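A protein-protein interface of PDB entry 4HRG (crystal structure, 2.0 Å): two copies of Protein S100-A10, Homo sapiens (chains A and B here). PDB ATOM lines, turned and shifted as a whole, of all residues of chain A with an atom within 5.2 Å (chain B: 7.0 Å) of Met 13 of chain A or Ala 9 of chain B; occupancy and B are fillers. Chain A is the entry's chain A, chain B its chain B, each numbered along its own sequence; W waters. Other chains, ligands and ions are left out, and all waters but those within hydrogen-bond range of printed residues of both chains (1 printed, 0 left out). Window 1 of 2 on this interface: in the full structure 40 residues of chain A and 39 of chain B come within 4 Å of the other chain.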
ATOM      1  N   HIS A   8      23.043  19.957   7.582  1.00  0.00           N
ATOM      2  CA  HIS A   8      23.744  21.023   6.878  1.00  0.00           C
ATOM      3  C   HIS A   8      23.186  22.369   7.322  1.00  0.00           C
ATOM      4  O   HIS A   8      23.941  23.324   7.497  1.00  0.00           O
ATOM      5  CB  HIS A   8      23.618  20.834   5.354  1.00  0.00           C
ATOM      6  CG  HIS A   8      24.292  21.903   4.548  1.00  0.00           C
ATOM      7  ND1 HIS A   8      23.611  22.978   4.017  1.00  0.00           N
ATOM      8  CD2 HIS A   8      25.583  22.057   4.175  1.00  0.00           C
ATOM      9  CE1 HIS A   8      24.453  23.747   3.353  1.00  0.00           C
ATOM     10  NE2 HIS A   8      25.659  23.215   3.438  1.00  0.00           N
ATOM     11  N   ALA A   9      21.865  22.453   7.507  1.00  0.00           N
ATOM     12  CA  ALA A   9      21.224  23.679   8.016  1.00  0.00           C
ATOM     13  C   ALA A   9      21.785  24.064   9.387  1.00  0.00           C
ATOM     14  O   ALA A   9      22.112  25.218   9.634  1.00  0.00           O
ATOM     15  CB  ALA A   9      19.684  23.497   8.095  1.00  0.00           C
ATOM     16  N   MET A  10      21.882  23.096  10.289  1.00  0.00           N
ATOM     17  CA  MET A  10      22.482  23.316  11.604  1.00  0.00           C
ATOM     18  C   MET A  10      23.905  23.795  11.497  1.00  0.00           C
ATOM     19  O   MET A  10      24.315  24.699  12.216  1.00  0.00           O
ATOM     20  CB  MET A  10      22.455  22.011  12.415  1.00  0.00           C
ATOM     21  CG  MET A  10      20.998  21.676  12.825  1.00  0.00           C
ATOM     22  SD  MET A  10      20.774  19.939  13.269  1.00  0.00           S
ATOM     23  CE  MET A  10      21.724  19.852  14.774  1.00  0.00           C
ATOM     24  N   GLU A  11      24.680  23.145  10.638  1.00  0.00           N
ATOM     25  CA  GLU A  11      26.067  23.529  10.426  1.00  0.00           C
ATOM     26  C   GLU A  11      26.167  24.962   9.915  1.00  0.00           C
ATOM     27  O   GLU A  11      27.047  25.728  10.324  1.00  0.00           O
ATOM     28  CB  GLU A  11      26.720  22.579   9.424  1.00  0.00           C
ATOM     29  CG  GLU A  11      28.233  22.619   9.507  1.00  0.00           C
ATOM     30  CD  GLU A  11      28.873  21.467   8.756  1.00  0.00           C
ATOM     31  OE1 GLU A  11      28.600  20.277   9.109  1.00  0.00           O
ATOM     32  OE2 GLU A  11      29.641  21.755   7.807  1.00  0.00           O
ATOM     33  N   THR A  12      25.254  25.334   9.030  1.00  0.00           N
ATOM     34  CA  THR A  12      25.203  26.683   8.497  1.00  0.00           C
ATOM     35  C   THR A  12      25.048  27.707   9.615  1.00  0.00           C
ATOM     36  O   THR A  12      25.722  28.746   9.638  1.00  0.00           O
ATOM     37  CB  THR A  12      24.010  26.817   7.531  1.00  0.00           C
ATOM     38  OG1 THR A  12      24.310  26.086   6.341  1.00  0.00           O
ATOM     39  CG2 THR A  12      23.780  28.268   7.172  1.00  0.00           C
ATOM     40  N   MET A  13      24.137  27.427  10.533  1.00  0.00           N
ATOM     41  CA  MET A  13      23.865  28.335  11.626  1.00  0.00           C
ATOM     42  C   MET A  13      25.025  28.422  12.605  1.00  0.00           C
ATOM     43  O   MET A  13      25.385  29.512  13.032  1.00  0.00           O
ATOM     44  CB  MET A  13      22.576  27.909  12.320  1.00  0.00           C
ATOM     45  CG  MET A  13      21.354  28.075  11.354  1.00  0.00           C
ATOM     46  SD  MET A  13      19.809  27.743  12.181  1.00  0.00           S
ATOM     47  CE  MET A  13      18.665  28.054  10.835  1.00  0.00           C
ATOM     48  N   MET A  14      25.638  27.291  12.921  1.00  0.00           N
ATOM     49  CA  MET A  14      26.836  27.261  13.753  1.00  0.00           C
ATOM     50  C   MET A  14      27.930  28.115  13.156  1.00  0.00           C
ATOM     51  O   MET A  14      28.500  28.994  13.806  1.00  0.00           O
ATOM     52  CB  MET A  14      27.425  25.824  13.808  1.00  0.00           C
ATOM     53  CG  MET A  14      27.137  24.950  15.025  1.00  0.00           C
ATOM     54  SD  MET A  14      28.494  23.837  15.583  1.00  0.00           S
ATOM     55  CE  MET A  14      29.475  23.562  14.099  1.00  0.00           C
ATOM     56  N   PHE A  15      28.267  27.809  11.913  1.00  0.00           N
ATOM     57  CA  PHE A  15      29.388  28.440  11.265  1.00  0.00           C
ATOM     58  C   PHE A  15      29.160  29.904  10.953  1.00  0.00           C
ATOM     59  O   PHE A  15      30.106  30.691  10.943  1.00  0.00           O
ATOM     60  CB  PHE A  15      29.743  27.681   9.995  1.00  0.00           C
ATOM     61  CG  PHE A  15      30.431  26.364  10.261  1.00  0.00           C
ATOM     62  CD1 PHE A  15      30.920  26.072  11.517  1.00  0.00           C
ATOM     63  CD2 PHE A  15      30.600  25.440   9.249  1.00  0.00           C
ATOM     64  CE1 PHE A  15      31.556  24.878  11.765  1.00  0.00           C
ATOM     65  CE2 PHE A  15      31.234  24.245   9.495  1.00  0.00           C
ATOM     66  CZ  PHE A  15      31.716  23.966  10.759  1.00  0.00           C
ATOM     67  N   THR A  16      27.920  30.272  10.676  1.00  0.00           N
ATOM     68  CA  THR A  16      27.575  31.674  10.476  1.00  0.00           C
ATOM     69  C   THR A  16      27.881  32.465  11.742  1.00  0.00           C
ATOM     70  O   THR A  16      28.472  33.530  11.670  1.00  0.00           O
ATOM     71  CB  THR A  16      26.080  31.881  10.070  1.00  0.00           C
ATOM     72  OG1 THR A  16      25.845  31.229   8.809  1.00  0.00           O
ATOM     73  CG2 THR A  16      25.777  33.432   9.911  1.00  0.00           C
ATOM     74  N   PHE A  17      27.471  31.957  12.899  1.00  0.00           N
ATOM     75  CA  PHE A  17      27.764  32.655  14.147  1.00  0.00           C
ATOM     76  C   PHE A  17      29.262  32.896  14.279  1.00  0.00           C
ATOM     77  O   PHE A  17      29.745  34.052  14.503  1.00  0.00           O
ATOM     78  CB  PHE A  17      27.281  31.809  15.338  1.00  0.00           C
ATOM     79  CG  PHE A  17      27.639  32.400  16.681  1.00  0.00           C
ATOM     80  CD1 PHE A  17      26.888  33.463  17.211  1.00  0.00           C
ATOM     81  CD2 PHE A  17      28.705  31.904  17.416  1.00  0.00           C
ATOM     82  CE1 PHE A  17      27.194  34.012  18.450  1.00  0.00           C
ATOM     83  CE2 PHE A  17      29.021  32.456  18.666  1.00  0.00           C
ATOM     84  CZ  PHE A  17      28.267  33.510  19.182  1.00  0.00           C
ATOM     85  N   PHE A  70      25.987  32.179  21.506  1.00  0.00           N
ATOM     86  CA  PHE A  70      25.372  31.380  20.451  1.00  0.00           C
ATOM     87  C   PHE A  70      23.926  31.090  20.770  1.00  0.00           C
ATOM     88  O   PHE A  70      23.050  31.145  19.889  1.00  0.00           O
ATOM     89  CB  PHE A  70      26.136  30.058  20.193  1.00  0.00           C
ATOM     90  CG  PHE A  70      25.529  29.265  19.107  1.00  0.00           C
ATOM     91  CD1 PHE A  70      25.663  29.673  17.788  1.00  0.00           C
ATOM     92  CD2 PHE A  70      24.700  28.177  19.398  1.00  0.00           C
ATOM     93  CE1 PHE A  70      25.015  28.989  16.757  1.00  0.00           C
ATOM     94  CE2 PHE A  70      24.111  27.483  18.393  1.00  0.00           C
ATOM     95  CZ  PHE A  70      24.247  27.888  17.060  1.00  0.00           C
ATOM     96  N   PHE A  73      22.036  34.031  20.009  1.00  0.00           N
ATOM     97  CA  PHE A  73      21.948  34.137  18.559  1.00  0.00           C
ATOM     98  C   PHE A  73      20.869  33.201  18.027  1.00  0.00           C
ATOM     99  O   PHE A  73      20.106  33.560  17.131  1.00  0.00           O
ATOM    100  CB  PHE A  73      23.296  33.810  17.913  1.00  0.00           C
ATOM    101  CG  PHE A  73      23.230  33.656  16.420  1.00  0.00           C
ATOM    102  CD1 PHE A  73      22.954  34.744  15.609  1.00  0.00           C
ATOM    103  CD2 PHE A  73      23.445  32.422  15.829  1.00  0.00           C
ATOM    104  CE1 PHE A  73      22.893  34.604  14.235  1.00  0.00           C
ATOM    105  CE2 PHE A  73      23.386  32.276  14.455  1.00  0.00           C
ATOM    106  CZ  PHE A  73      23.110  33.369  13.657  1.00  0.00           C
ATOM    107  N   PHE A  74      20.810  31.999  18.591  1.00  0.00           N
ATOM    108  CA  PHE A  74      19.807  31.029  18.210  1.00  0.00           C
ATOM    109  C   PHE A  74      18.383  31.479  18.547  1.00  0.00           C
ATOM    110  O   PHE A  74      17.439  31.127  17.833  1.00  0.00           O
ATOM    111  CB  PHE A  74      20.075  29.635  18.799  1.00  0.00           C
ATOM    112  CG  PHE A  74      19.657  28.542  17.880  1.00  0.00           C
ATOM    113  CD1 PHE A  74      20.510  28.096  16.880  1.00  0.00           C
ATOM    114  CD2 PHE A  74      18.376  28.005  17.958  1.00  0.00           C
ATOM    115  CE1 PHE A  74      20.117  27.097  16.007  1.00  0.00           C
ATOM    116  CE2 PHE A  74      17.964  27.007  17.068  1.00  0.00           C
ATOM    117  CZ  PHE A  74      18.848  26.548  16.103  1.00  0.00           C
ATOM    118  N   ILE A  77      17.169  33.494  15.647  1.00  0.00           N
ATOM    119  CA  ILE A  77      16.723  32.633  14.549  1.00  0.00           C
ATOM    120  C   ILE A  77      15.396  31.972  14.909  1.00  0.00           C
ATOM    121  O   ILE A  77      14.512  31.799  14.046  1.00  0.00           O
ATOM    122  CB  ILE A  77      17.770  31.530  14.231  1.00  0.00           C
ATOM    123  CG1 ILE A  77      19.119  32.182  13.894  1.00  0.00           C
ATOM    124  CG2 ILE A  77      17.302  30.662  13.057  1.00  0.00           C
ATOM    125  CD1 ILE A  77      19.021  33.319  12.890  1.00  0.00           C
ATOM    126  N   SER B   4      21.179  33.677   0.370  1.00  0.00           N
ATOM    127  CA  SER B   4      21.655  33.769   1.742  1.00  0.00           C
ATOM    128  C   SER B   4      21.643  32.365   2.360  1.00  0.00           C
ATOM    129  O   SER B   4      20.649  31.632   2.257  1.00  0.00           O
ATOM    130  CB  SER B   4      20.747  34.678   2.555  1.00  0.00           C
ATOM    131  OG  SER B   4      20.735  34.282   3.918  1.00  0.00           O
ATOM    132  N   GLN B   5      22.743  31.973   3.002  1.00  0.00           N
ATOM    133  CA  GLN B   5      22.796  30.655   3.624  1.00  0.00           C
ATOM    134  C   GLN B   5      21.837  30.548   4.807  1.00  0.00           C
ATOM    135  O   GLN B   5      21.200  29.492   5.021  1.00  0.00           O
ATOM    136  CB  GLN B   5      24.238  30.343   4.064  1.00  0.00           C
ATOM    137  CG  GLN B   5      25.176  30.083   2.904  1.00  0.00           C
ATOM    138  CD  GLN B   5      26.620  29.866   3.372  1.00  0.00           C
ATOM    139  OE1 GLN B   5      26.910  28.922   4.112  1.00  0.00           O
ATOM    140  NE2 GLN B   5      27.522  30.753   2.954  1.00  0.00           N
ATOM    141  N   MET B   6      21.717  31.621   5.590  1.00  0.00           N
ATOM    142  CA  MET B   6      20.802  31.574   6.738  1.00  0.00           C
ATOM    143  C   MET B   6      19.346  31.427   6.272  1.00  0.00           C
ATOM    144  O   MET B   6      18.586  30.655   6.850  1.00  0.00           O
ATOM    145  CB  MET B   6      20.936  32.788   7.648  1.00  0.00           C
ATOM    146  CG  MET B   6      22.248  32.851   8.472  1.00  0.00           C
ATOM    147  SD  MET B   6      22.223  31.411   9.591  1.00  0.00           S
ATOM    148  CE  MET B   6      20.573  31.529  10.312  1.00  0.00           C
ATOM    149  N   GLU B   7      18.943  32.178   5.250  1.00  0.00           N
ATOM    150  CA  GLU B   7      17.554  32.085   4.767  1.00  0.00           C
ATOM    151  C   GLU B   7      17.314  30.694   4.210  1.00  0.00           C
ATOM    152  O   GLU B   7      16.250  30.108   4.389  1.00  0.00           O
ATOM    153  CB  GLU B   7      17.296  33.159   3.696  1.00  0.00           C
ATOM    154  CG  GLU B   7      17.171  34.583   4.300  1.00  0.00           C
ATOM    155  CD  GLU B   7      17.054  35.685   3.249  1.00  0.00           C
ATOM    156  OE1 GLU B   7      17.429  35.465   2.067  1.00  0.00           O
ATOM    157  OE2 GLU B   7      16.595  36.792   3.619  1.00  0.00           O
ATOM    158  N   HIS B   8      18.319  30.150   3.532  1.00  0.00           N
ATOM    159  CA  HIS B   8      18.198  28.767   3.070  1.00  0.00           C
ATOM    160  C   HIS B   8      18.007  27.784   4.239  1.00  0.00           C
ATOM    161  O   HIS B   8      17.143  26.893   4.181  1.00  0.00           O
ATOM    162  CB  HIS B   8      19.414  28.356   2.248  1.00  0.00           C
ATOM    163  CG  HIS B   8      19.300  26.984   1.669  1.00  0.00           C
ATOM    164  ND1 HIS B   8      18.831  26.750   0.387  1.00  0.00           N
ATOM    165  CD2 HIS B   8      19.552  25.761   2.196  1.00  0.00           C
ATOM    166  CE1 HIS B   8      18.820  25.455   0.156  1.00  0.00           C
ATOM    167  NE2 HIS B   8      19.258  24.827   1.239  1.00  0.00           N
ATOM    168  N   ALA B   9      18.807  27.936   5.296  1.00  0.00           N
ATOM    169  CA  ALA B   9      18.721  27.043   6.453  1.00  0.00           C
ATOM    170  C   ALA B   9      17.349  27.126   7.128  1.00  0.00           C
ATOM    171  O   ALA B   9      16.814  26.109   7.589  1.00  0.00           O
ATOM    172  CB  ALA B   9      19.843  27.365   7.489  1.00  0.00           C
ATOM    173  N   MET B  10      16.780  28.331   7.206  1.00  0.00           N
ATOM    174  CA  MET B  10      15.432  28.501   7.802  1.00  0.00           C
ATOM    175  C   MET B  10      14.374  27.767   6.994  1.00  0.00           C
ATOM    176  O   MET B  10      13.473  27.115   7.565  1.00  0.00           O
ATOM    177  CB  MET B  10      15.089  29.990   7.924  1.00  0.00           C
ATOM    178  CG  MET B  10      15.991  30.705   8.941  1.00  0.00           C
ATOM    179  SD  MET B  10      16.023  32.507   8.839  1.00  0.00           S
ATOM    180  CE  MET B  10      14.408  32.909   9.488  1.00  0.00           C
ATOM    181  N   GLU B  11      14.461  27.878   5.666  1.00  0.00           N
ATOM    182  CA  GLU B  11      13.533  27.187   4.780  1.00  0.00           C
ATOM    183  C   GLU B  11      13.616  25.699   5.008  1.00  0.00           C
ATOM    184  O   GLU B  11      12.588  24.999   4.982  1.00  0.00           O
ATOM    185  CB  GLU B  11      13.845  27.481   3.298  1.00  0.00           C
ATOM    186  CG  GLU B  11      13.301  28.811   2.803  1.00  0.00           C
ATOM    187  CD  GLU B  11      13.780  29.160   1.408  1.00  0.00           C
ATOM    188  OE1 GLU B  11      13.292  30.181   0.864  1.00  0.00           O
ATOM    189  OE2 GLU B  11      14.644  28.430   0.846  1.00  0.00           O
ATOM    190  N   THR B  12      14.838  25.198   5.197  1.00  0.00           N
ATOM    191  CA  THR B  12      15.025  23.775   5.417  1.00  0.00           C
ATOM    192  C   THR B  12      14.280  23.346   6.661  1.00  0.00           C
ATOM    193  O   THR B  12      13.592  22.321   6.666  1.00  0.00           O
ATOM    194  CB  THR B  12      16.526  23.379   5.602  1.00  0.00           C
ATOM    195  OG1 THR B  12      17.227  23.572   4.382  1.00  0.00           O
ATOM    196  CG2 THR B  12      16.625  21.907   5.905  1.00  0.00           C
ATOM    197  N   MET B  13      14.429  24.102   7.731  1.00  0.00           N
ATOM    198  CA  MET B  13      13.785  23.765   8.998  1.00  0.00           C
ATOM    199  C   MET B  13      12.266  23.843   8.935  1.00  0.00           C
ATOM    200  O   MET B  13      11.554  22.962   9.445  1.00  0.00           O
ATOM    201  CB  MET B  13      14.321  24.697  10.097  1.00  0.00           C
ATOM    202  CG  MET B  13      15.832  24.506  10.300  1.00  0.00           C
ATOM    203  SD  MET B  13      16.352  25.265  11.825  1.00  0.00           S
ATOM    204  CE  MET B  13      15.935  26.978  11.531  1.00  0.00           C
ATOM    205  N   MET B  14      11.761  24.900   8.319  1.00  0.00           N
ATOM    206  CA  MET B  14      10.307  25.024   8.121  1.00  0.00           C
ATOM    207  C   MET B  14       9.724  23.937   7.256  1.00  0.00           C
ATOM    208  O   MET B  14       8.690  23.338   7.602  1.00  0.00           O
ATOM    209  CB  MET B  14       9.977  26.396   7.481  1.00  0.00           C
ATOM    210  CG  MET B  14       8.533  26.769   7.442  1.00  0.00           C
ATOM    211  SD  MET B  14       8.342  28.486   6.839  1.00  0.00           S
ATOM    212  CE  MET B  14       8.338  28.134   5.075  1.00  0.00           C
ATOM    213  N   PHE B  74      11.097  23.340  16.869  1.00  0.00           N
ATOM    214  CA  PHE B  74      12.271  24.200  16.853  1.00  0.00           C
ATOM    215  C   PHE B  74      13.100  24.042  18.146  1.00  0.00           C
ATOM    216  O   PHE B  74      14.323  24.181  18.132  1.00  0.00           O
ATOM    217  CB  PHE B  74      11.890  25.664  16.611  1.00  0.00           C
ATOM    218  CG  PHE B  74      13.013  26.472  15.998  1.00  0.00           C
ATOM    219  CD1 PHE B  74      13.141  26.555  14.623  1.00  0.00           C
ATOM    220  CD2 PHE B  74      13.961  27.076  16.789  1.00  0.00           C
ATOM    221  CE1 PHE B  74      14.173  27.267  14.042  1.00  0.00           C
ATOM    222  CE2 PHE B  74      15.016  27.815  16.216  1.00  0.00           C
ATOM    223  CZ  PHE B  74      15.104  27.896  14.822  1.00  0.00           C
ATOM    224  N   ILE B  77      15.600  21.335  17.622  1.00  0.00           N
ATOM    225  CA  ILE B  77      16.710  21.771  16.783  1.00  0.00           C
ATOM    226  C   ILE B  77      17.648  22.647  17.607  1.00  0.00           C
ATOM    227  O   ILE B  77      18.881  22.552  17.495  1.00  0.00           O
ATOM    228  CB  ILE B  77      16.199  22.565  15.584  1.00  0.00           C
ATOM    229  CG1 ILE B  77      15.189  21.712  14.793  1.00  0.00           C
ATOM    230  CG2 ILE B  77      17.357  22.988  14.688  1.00  0.00           C
ATOM    231  CD1 ILE B  77      15.688  20.305  14.526  1.00  0.00           C
ATOM    232  N   THR B  81      21.446  21.854  18.334  1.00  0.00           N
ATOM    233  CA  THR B  81      22.449  22.736  17.727  1.00  0.00           C
ATOM    234  C   THR B  81      23.289  23.430  18.801  1.00  0.00           C
ATOM    235  O   THR B  81      24.492  23.679  18.619  1.00  0.00           O
ATOM    236  CB  THR B  81      21.807  23.785  16.802  1.00  0.00           C
ATOM    237  OG1 THR B  81      20.967  23.122  15.860  1.00  0.00           O
ATOM    238  CG2 THR B  81      22.874  24.529  16.036  1.00  0.00           C
ATOM    239  N   ASN B  85      27.284  23.050  19.242  1.00  0.00           N
ATOM    240  CA  ASN B  85      28.176  24.198  19.252  1.00  0.00           C
ATOM    241  C   ASN B  85      29.095  24.171  20.457  1.00  0.00           C
ATOM    242  O   ASN B  85      30.284  24.532  20.369  1.00  0.00           O
ATOM    243  CB  ASN B  85      27.366  25.490  19.307  1.00  0.00           C
ATOM    244  CG  ASN B  85      28.252  26.706  19.248  1.00  0.00           C
ATOM    245  OD1 ASN B  85      28.915  26.940  18.238  1.00  0.00           O
ATOM    246  ND2 ASN B  85      28.293  27.473  20.333  1.00  0.00           N
HETATM  247  O   HOH W   1      22.498  27.089   3.923  1.00  0.00           O
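SD of Met 6 of chain B is in hydrogen-bond range of OG1 of Thr 16 of chain A, at 3.7 Å.
The side-chain hydroxyl (OG1) of Thr 81 of chain B is in hydrogen-bond range of the backbone carbonyl oxygen (O) of Ile 77 of chain B. OG1 of Thr 16 of chain A lies within hydrogen-bond range of O of Thr 12 of chain A, at 2.6 Å. OG of Ser 4 of chain B lies within hydrogen-bond range of N of Met 6 of chain B, 3.3 Å away. The backbone carbonyl oxygen (O) of His 8 of chain A is in hydrogen-bond range of the side-chain hydroxyl (OG1) of Thr 12 of chain A.
Among the printed residues, merely in contact across the chains: Ala 9 of chain A with Ala 9 of chain B (3.8 Å), Met 10 of chain A with Thr 81 of chain B (3.4 Å), Thr 12 of chain A with Gln 5 of chain B (3.6 Å), Met 13 of chain A with Met 6 of chain B (3.7 Å), Met 13 of chain A with Ala 9 of chain B (3.6 Å), Met 13 of chain A with Met 13 of chain B (3.0 Å), Met 14 of chain A with Asn 85 of chain B (3.7 Å), Phe 70 of chain A with Thr 81 of chain B (3.8 Å), Phe 70 of chain A with Asn 85 of chain B (3.4 Å), Phe 74 of chain A with Phe 74 of chain B (3.2 Å), Phe 74 of chain A with Thr 81 of chain B (3.8 Å), Ile 77 of chain A with Met 6 of chain B (3.5 Å) and Ile 77 of chain A with Phe 74 of chain B (3.9 Å).
Met 13 of chain A touches just these residues of chain B: Met 6, Ala 9 and Met 13. Of chain A, only Ala 9 and Met 13 come within 4 Å of Ala 9 of chain B. Printed residues of chain A within 4 Å of Met 13 of chain B: Met 13. Of the printed residues of chain B, Ile 77 of chain A touches Met 6 (3.5 Å) and Phe 74 (3.9 Å). Of the printed residues of chain B, Thr 12 of chain A touches Gln 5 (3.6 Å). His 8 of chain B touches none of the printed residues of chain A.
Of the 14 printed residues of chain A, 9 touch a printed residue of chain B. Hydrophobic or aromatic side chains of chain A within 4 Å of the printed part of chain B: Ala 9, Met 10, Met 13, Met 14, Phe 70, Phe 74 and Ile 77. Along chain A the printed residues that touch a printed residue of chain B span positions 9 to 77. Of the 15 printed residues of chain B, 7 touch a printed residue of chain A. Printed residues of chain B that touch a printed residue of chain A: Gln 5, Met 6, Ala 9, Met 13, Phe 74, Thr 81 and Asn 85. Hydrophobic or aromatic side chains of chain B within 4 Å of the printed part of chain A: Met 6, Ala 9, Met 13 and Phe 74. Among the printed residues, no Asp or Glu carboxylate lies within 4 Å of a Lys or Arg side-chain nitrogen of the other chain.
Ala 9 of chain B touches its own counterpart, Ala 9 of chain A. Met 13 of chain A touches Ala 9 of chain B, but with the chains exchanged Ala 9 of chain A does not touch Met 13 of chain B (4.6 Å). Met 13 of chain A touches its own counterpart, Met 13 of chain B. Phe 74 of chain B touches its own counterpart, Phe 74 of chain A. 9 positions are printed for both chains.
Water W1 bridges the backbone carbonyl oxygen (O) of Gln 5 of chain B and the side-chain hydroxyl (OG1) of Thr 12 of chain A.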
